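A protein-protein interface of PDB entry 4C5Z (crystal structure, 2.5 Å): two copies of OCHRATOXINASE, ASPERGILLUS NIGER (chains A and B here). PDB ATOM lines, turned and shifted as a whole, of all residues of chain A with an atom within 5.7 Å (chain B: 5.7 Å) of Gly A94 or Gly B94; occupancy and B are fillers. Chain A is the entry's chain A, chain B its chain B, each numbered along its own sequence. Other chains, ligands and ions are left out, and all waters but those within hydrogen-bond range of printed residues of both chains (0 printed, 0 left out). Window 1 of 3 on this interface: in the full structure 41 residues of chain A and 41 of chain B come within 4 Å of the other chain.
A ring nitrogen (ND1) of His A89 sits at hydrogen-bond distance from the backbone NH of Ala A91 (3.1 Å).
N of Ala B91 is in hydrogen-bond range of ND1 of His B89, 3.1 Å away.
The side-chain hydroxyl of Ser A93 is in hydrogen-bond range of the backbone carbonyl oxygen of His A89.
OG of Ser B93 is in hydrogen-bond range of O of His B89.
His A89 touches Pro B90.
O of Pro A90 touches O of Pro B90 (3.9 Å).
O of Pro A90 touches CA of Ala B91 (3.4 Å).
Ala A91 touches Pro B90.
Ala A91 touches Gly B94 (O to CA, 3.4 Å).
Gly A94 touches Ala B91 (CA to O, 3.4 Å).
C of Gly A94 touches C of Gly B94 (3.6 Å).
Gly B94 touches Ala A95.
Ala B95 touches Ala A95 (N to N, 3.8 Å).
O of Ala A95 touches CB of Ala B98 (3.95 Å).
Of the printed residues of chain B, His A89 touches Pro B90 (3.9 Å).
Of the printed residues of chain B, Pro A90 touches His B89, Pro B90 and Ala B91.
Of the printed residues of chain B, Ala A91 touches Pro B90 and Gly B94.
Ser A93 touches none of the printed residues of chain B.
Gly A94 touches just these residues of chain B: Ala B91, Gly B94 and Ala B95.
Of the printed residues of chain A, Ala B91 touches Pro A90 and Gly A94.
Gly B94 touches just these residues of chain A: Ala A91, Gly A94 and Ala A95.
Printed residues of chain A that touch a printed residue of chain B: His A89, Pro A90, Ala A91, Gly A94, Ala A95 and Ala A98.
Hydrophobic or aromatic side chains of chain A within 4 Å of the printed part of chain B: His A89, Pro A90, Ala A91, Ala A95 and Ala A98.
Among the printed residues, 14 pairs touch across the chains.
Among the printed residues, no Asp or Glu carboxylate lies within 4 Å of a Lys or Arg side-chain nitrogen of the other chain.
His A89 touches Pro B90, and with the chains exchanged Pro A90 touches His B89.
Pro B90 touches its own counterpart, Pro A90.
Gly A94 touches its own counterpart, Gly B94.
Gly A94 touches Ala B95, and with the chains exchanged Ala A95 touches Gly B94.
Positions printed for both chains: 74, 89, 90, 91, 92, 93, 94, 95, 96, 97, 98, 99 and 122.
Of the 14 pairs that touch across the chains among the printed residues, 14 have their exchanged pair printed and touching as well.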
ATOM      1  N   GLY A  74      31.894  16.620  28.412  1.00  0.00           N
ATOM      2  CA  GLY A  74      31.818  17.283  27.099  1.00  0.00           C
ATOM      3  C   GLY A  74      31.275  18.707  27.098  1.00  0.00           C
ATOM      4  O   GLY A  74      30.692  19.157  26.129  1.00  0.00           O
ATOM      5  N   HIS A  89      23.997  21.370  26.446  1.00  0.00           N
ATOM      6  CA  HIS A  89      23.027  20.425  25.909  1.00  0.00           C
ATOM      7  C   HIS A  89      23.714  19.087  25.696  1.00  0.00           C
ATOM      8  O   HIS A  89      24.858  19.044  25.245  1.00  0.00           O
ATOM      9  CB  HIS A  89      22.466  20.938  24.581  1.00  0.00           C
ATOM     10  CG  HIS A  89      21.264  20.196  24.105  1.00  0.00           C
ATOM     11  ND1 HIS A  89      21.333  18.940  23.567  1.00  0.00           N
ATOM     12  CD2 HIS A  89      19.966  20.563  24.021  1.00  0.00           C
ATOM     13  CE1 HIS A  89      20.129  18.542  23.209  1.00  0.00           C
ATOM     14  NE2 HIS A  89      19.281  19.515  23.465  1.00  0.00           N
ATOM     15  N   PRO A  90      23.037  17.978  26.003  1.00  0.00           N
ATOM     16  CA  PRO A  90      23.815  16.755  25.967  1.00  0.00           C
ATOM     17  C   PRO A  90      24.242  16.306  24.598  1.00  0.00           C
ATOM     18  O   PRO A  90      25.200  15.581  24.483  1.00  0.00           O
ATOM     19  CB  PRO A  90      22.894  15.752  26.630  1.00  0.00           C
ATOM     20  CG  PRO A  90      22.097  16.581  27.565  1.00  0.00           C
ATOM     21  CD  PRO A  90      21.811  17.816  26.779  1.00  0.00           C
ATOM     22  N   ALA A  91      23.578  16.776  23.556  1.00  0.00           N
ATOM     23  CA  ALA A  91      24.011  16.477  22.197  1.00  0.00           C
ATOM     24  C   ALA A  91      25.371  17.082  21.937  1.00  0.00           C
ATOM     25  O   ALA A  91      26.216  16.446  21.310  1.00  0.00           O
ATOM     26  CB  ALA A  91      22.994  16.974  21.173  1.00  0.00           C
ATOM     27  N   SER A  92      25.591  18.307  22.388  1.00  0.00           N
ATOM     28  CA  SER A  92      26.914  18.891  22.284  1.00  0.00           C
ATOM     29  C   SER A  92      27.903  18.021  23.073  1.00  0.00           C
ATOM     30  O   SER A  92      28.964  17.667  22.583  1.00  0.00           O
ATOM     31  CB  SER A  92      26.925  20.291  22.839  1.00  0.00           C
ATOM     32  OG  SER A  92      25.948  21.089  22.209  1.00  0.00           O
ATOM     33  N   SER A  93      27.548  17.653  24.289  1.00  0.00           N
ATOM     34  CA  SER A  93      28.461  16.880  25.129  1.00  0.00           C
ATOM     35  C   SER A  93      28.863  15.604  24.437  1.00  0.00           C
ATOM     36  O   SER A  93      30.025  15.218  24.468  1.00  0.00           O
ATOM     37  CB  SER A  93      27.810  16.536  26.460  1.00  0.00           C
ATOM     38  OG  SER A  93      27.340  17.699  27.143  1.00  0.00           O
ATOM     39  N   GLY A  94      27.885  14.944  23.815  1.00  0.00           N
ATOM     40  CA  GLY A  94      28.100  13.660  23.190  1.00  0.00           C
ATOM     41  C   GLY A  94      29.025  13.772  22.009  1.00  0.00           C
ATOM     42  O   GLY A  94      29.903  12.926  21.827  1.00  0.00           O
ATOM     43  N   ALA A  95      28.836  14.804  21.188  1.00  0.00           N
ATOM     44  CA  ALA A  95      29.723  15.006  20.054  1.00  0.00           C
ATOM     45  C   ALA A  95      31.146  15.089  20.555  1.00  0.00           C
ATOM     46  O   ALA A  95      32.033  14.365  20.083  1.00  0.00           O
ATOM     47  CB  ALA A  95      29.359  16.261  19.310  1.00  0.00           C
ATOM     48  N   ARG A  96      31.361  15.958  21.533  1.00  0.00           N
ATOM     49  CA  ARG A  96      32.704  16.212  22.020  1.00  0.00           C
ATOM     50  C   ARG A  96      33.310  14.945  22.630  1.00  0.00           C
ATOM     51  O   ARG A  96      34.488  14.660  22.427  1.00  0.00           O
ATOM     52  CB  ARG A  96      32.714  17.339  23.050  1.00  0.00           C
ATOM     53  CG  ARG A  96      32.360  18.688  22.497  1.00  0.00           C
ATOM     54  CD  ARG A  96      32.850  19.764  23.435  1.00  0.00           C
ATOM     55  NE  ARG A  96      32.422  21.097  23.014  1.00  0.00           N
ATOM     56  CZ  ARG A  96      31.239  21.647  23.276  1.00  0.00           C
ATOM     57  NH1 ARG A  96      30.338  21.015  24.016  1.00  0.00           N
ATOM     58  NH2 ARG A  96      30.945  22.844  22.773  1.00  0.00           N
ATOM     59  N   LEU A  97      32.508  14.189  23.370  1.00  0.00           N
ATOM     60  CA  LEU A  97      32.994  12.961  24.006  1.00  0.00           C
ATOM     61  C   LEU A  97      33.418  11.892  22.972  1.00  0.00           C
ATOM     62  O   LEU A  97      34.246  11.023  23.283  1.00  0.00           O
ATOM     63  CB  LEU A  97      31.933  12.412  24.951  1.00  0.00           C
ATOM     64  CG  LEU A  97      31.683  13.288  26.177  1.00  0.00           C
ATOM     65  CD1 LEU A  97      30.403  12.904  26.887  1.00  0.00           C
ATOM     66  CD2 LEU A  97      32.835  13.211  27.153  1.00  0.00           C
ATOM     67  N   ALA A  98      32.876  11.973  21.750  1.00  0.00           N
ATOM     68  CA  ALA A  98      33.259  11.074  20.681  1.00  0.00           C
ATOM     69  C   ALA A  98      34.681  11.350  20.268  1.00  0.00           C
ATOM     70  O   ALA A  98      35.485  10.409  20.156  1.00  0.00           O
ATOM     71  CB  ALA A  98      32.327  11.172  19.510  1.00  0.00           C
ATOM     72  N   ARG A  99      35.044  12.613  20.097  1.00  0.00           N
ATOM     73  CA  ARG A  99      36.453  12.927  19.832  1.00  0.00           C
ATOM     74  C   ARG A  99      37.355  12.391  20.964  1.00  0.00           C
ATOM     75  O   ARG A  99      38.433  11.836  20.734  1.00  0.00           O
ATOM     76  CB  ARG A  99      36.653  14.411  19.711  1.00  0.00           C
ATOM     77  CG  ARG A  99      38.113  14.813  19.537  1.00  0.00           C
ATOM     78  CD  ARG A  99      38.616  14.340  18.195  1.00  0.00           C
ATOM     79  NE  ARG A  99      39.959  14.774  17.865  1.00  0.00           N
ATOM     80  CZ  ARG A  99      40.288  15.966  17.391  1.00  0.00           C
ATOM     81  NH1 ARG A  99      39.370  16.901  17.211  1.00  0.00           N
ATOM     82  NH2 ARG A  99      41.558  16.213  17.095  1.00  0.00           N
ATOM     83  N   VAL A 122      27.048   7.301  26.100  1.00  0.00           N
ATOM     84  CA  VAL A 122      28.031   7.292  25.031  1.00  0.00           C
ATOM     85  C   VAL A 122      28.515   5.863  24.738  1.00  0.00           C
ATOM     86  O   VAL A 122      28.816   5.525  23.593  1.00  0.00           O
ATOM     87  CB  VAL A 122      29.180   8.290  25.343  1.00  0.00           C
ATOM     88  CG1 VAL A 122      30.368   8.105  24.403  1.00  0.00           C
ATOM     89  CG2 VAL A 122      28.662   9.727  25.285  1.00  0.00           C
ATOM     90  N   GLY B  74      20.708  10.850  15.210  1.00  0.00           N
ATOM     91  CA  GLY B  74      21.600   9.930  15.947  1.00  0.00           C
ATOM     92  C   GLY B  74      20.910   8.898  16.822  1.00  0.00           C
ATOM     93  O   GLY B  74      21.454   8.469  17.836  1.00  0.00           O
ATOM     94  N   HIS B  89      18.657   9.220  24.275  1.00  0.00           N
ATOM     95  CA  HIS B  89      19.276  10.290  25.066  1.00  0.00           C
ATOM     96  C   HIS B  89      20.164  11.144  24.161  1.00  0.00           C
ATOM     97  O   HIS B  89      20.845  10.621  23.289  1.00  0.00           O
ATOM     98  CB  HIS B  89      20.099   9.712  26.207  1.00  0.00           C
ATOM     99  CG  HIS B  89      20.490  10.724  27.239  1.00  0.00           C
ATOM    100  ND1 HIS B  89      21.467  11.662  27.023  1.00  0.00           N
ATOM    101  CD2 HIS B  89      20.063  10.923  28.510  1.00  0.00           C
ATOM    102  CE1 HIS B  89      21.633  12.394  28.111  1.00  0.00           C
ATOM    103  NE2 HIS B  89      20.793  11.962  29.029  1.00  0.00           N
ATOM    104  N   PRO B  90      20.163  12.454  24.360  1.00  0.00           N
ATOM    105  CA  PRO B  90      20.841  13.212  23.313  1.00  0.00           C
ATOM    106  C   PRO B  90      22.347  13.053  23.315  1.00  0.00           C
ATOM    107  O   PRO B  90      22.980  13.308  22.301  1.00  0.00           O
ATOM    108  CB  PRO B  90      20.405  14.650  23.589  1.00  0.00           C
ATOM    109  CG  PRO B  90      19.056  14.494  24.190  1.00  0.00           C
ATOM    110  CD  PRO B  90      19.213  13.290  25.096  1.00  0.00           C
ATOM    111  N   ALA B  91      22.923  12.613  24.431  1.00  0.00           N
ATOM    112  CA  ALA B  91      24.353  12.330  24.477  1.00  0.00           C
ATOM    113  C   ALA B  91      24.694  11.197  23.542  1.00  0.00           C
ATOM    114  O   ALA B  91      25.699  11.258  22.844  1.00  0.00           O
ATOM    115  CB  ALA B  91      24.808  12.018  25.896  1.00  0.00           C
ATOM    116  N   SER B  92      23.845  10.170  23.508  1.00  0.00           N
ATOM    117  CA  SER B  92      24.020   9.102  22.525  1.00  0.00           C
ATOM    118  C   SER B  92      23.906   9.690  21.132  1.00  0.00           C
ATOM    119  O   SER B  92      24.747   9.436  20.280  1.00  0.00           O
ATOM    120  CB  SER B  92      22.973   8.013  22.706  1.00  0.00           C
ATOM    121  OG  SER B  92      22.977   7.532  24.033  1.00  0.00           O
ATOM    122  N   SER B  93      22.889  10.507  20.905  1.00  0.00           N
ATOM    123  CA  SER B  93      22.674  11.074  19.569  1.00  0.00           C
ATOM    124  C   SER B  93      23.886  11.861  19.100  1.00  0.00           C
ATOM    125  O   SER B  93      24.297  11.738  17.952  1.00  0.00           O
ATOM    126  CB  SER B  93      21.460  12.007  19.539  1.00  0.00           C
ATOM    127  OG  SER B  93      20.291  11.354  20.012  1.00  0.00           O
ATOM    128  N   GLY B  94      24.456  12.652  20.003  1.00  0.00           N
ATOM    129  CA  GLY B  94      25.582  13.510  19.671  1.00  0.00           C
ATOM    130  C   GLY B  94      26.819  12.722  19.310  1.00  0.00           C
ATOM    131  O   GLY B  94      27.528  13.059  18.376  1.00  0.00           O
ATOM    132  N   ALA B  95      27.088  11.665  20.060  1.00  0.00           N
ATOM    133  CA  ALA B  95      28.219  10.831  19.744  1.00  0.00           C
ATOM    134  C   ALA B  95      28.084  10.339  18.314  1.00  0.00           C
ATOM    135  O   ALA B  95      29.026  10.457  17.508  1.00  0.00           O
ATOM    136  CB  ALA B  95      28.298   9.663  20.688  1.00  0.00           C
ATOM    137  N   ARG B  96      26.919   9.787  18.002  1.00  0.00           N
ATOM    138  CA  ARG B  96      26.719   9.136  16.714  1.00  0.00           C
ATOM    139  C   ARG B  96      26.820  10.179  15.613  1.00  0.00           C
ATOM    140  O   ARG B  96      27.422   9.929  14.574  1.00  0.00           O
ATOM    141  CB  ARG B  96      25.375   8.392  16.665  1.00  0.00           C
ATOM    142  CG  ARG B  96      25.304   7.148  17.576  1.00  0.00           C
ATOM    143  CD  ARG B  96      24.217   6.073  17.274  1.00  0.00           C
ATOM    144  NE  ARG B  96      23.267   6.061  18.371  1.00  0.00           N
ATOM    145  CZ  ARG B  96      23.176   5.142  19.340  1.00  0.00           C
ATOM    146  NH1 ARG B  96      23.947   4.077  19.396  1.00  0.00           N
ATOM    147  NH2 ARG B  96      22.271   5.298  20.278  1.00  0.00           N
ATOM    148  N   LEU B  97      26.281  11.369  15.859  1.00  0.00           N
ATOM    149  CA  LEU B  97      26.330  12.438  14.866  1.00  0.00           C
ATOM    150  C   LEU B  97      27.751  12.932  14.561  1.00  0.00           C
ATOM    151  O   LEU B  97      28.022  13.453  13.478  1.00  0.00           O
ATOM    152  CB  LEU B  97      25.444  13.595  15.304  1.00  0.00           C
ATOM    153  CG  LEU B  97      23.943  13.263  15.302  1.00  0.00           C
ATOM    154  CD1 LEU B  97      23.135  14.300  16.062  1.00  0.00           C
ATOM    155  CD2 LEU B  97      23.390  13.155  13.882  1.00  0.00           C
ATOM    156  N   ALA B  98      28.663  12.740  15.505  1.00  0.00           N
ATOM    157  CA  ALA B  98      30.055  13.097  15.275  1.00  0.00           C
ATOM    158  C   ALA B  98      30.676  12.192  14.217  1.00  0.00           C
ATOM    159  O   ALA B  98      31.358  12.663  13.325  1.00  0.00           O
ATOM    160  CB  ALA B  98      30.842  13.014  16.565  1.00  0.00           C
ATOM    161  N   ARG B  99      30.439  10.885  14.311  1.00  0.00           N
ATOM    162  CA  ARG B  99      30.891   9.980  13.249  1.00  0.00           C
ATOM    163  C   ARG B  99      30.323  10.420  11.899  1.00  0.00           C
ATOM    164  O   ARG B  99      31.021  10.413  10.883  1.00  0.00           O
ATOM    165  CB  ARG B  99      30.457   8.545  13.515  1.00  0.00           C
ATOM    166  CG  ARG B  99      30.827   7.572  12.405  1.00  0.00           C
ATOM    167  CD  ARG B  99      32.331   7.410  12.357  1.00  0.00           C
ATOM    168  NE  ARG B  99      32.794   6.411  11.399  1.00  0.00           N
ATOM    169  CZ  ARG B  99      32.826   5.099  11.604  1.00  0.00           C
ATOM    170  NH1 ARG B  99      32.373   4.598  12.729  1.00  0.00           N
ATOM    171  NH2 ARG B  99      33.284   4.290  10.648  1.00  0.00           N
ATOM    172  N   VAL B 122      25.158  20.282  17.817  1.00  0.00           N
ATOM    173  CA  VAL B 122      26.360  19.621  17.323  1.00  0.00           C
ATOM    174  C   VAL B 122      27.294  20.613  16.603  1.00  0.00           C
ATOM    175  O   VAL B 122      28.516  20.483  16.666  1.00  0.00           O
ATOM    176  CB  VAL B 122      25.979  18.405  16.440  1.00  0.00           C
ATOM    177  CG1 VAL B 122      27.174  17.850  15.693  1.00  0.00           C
ATOM    178  CG2 VAL B 122      25.343  17.330  17.320  1.00  0.00           C
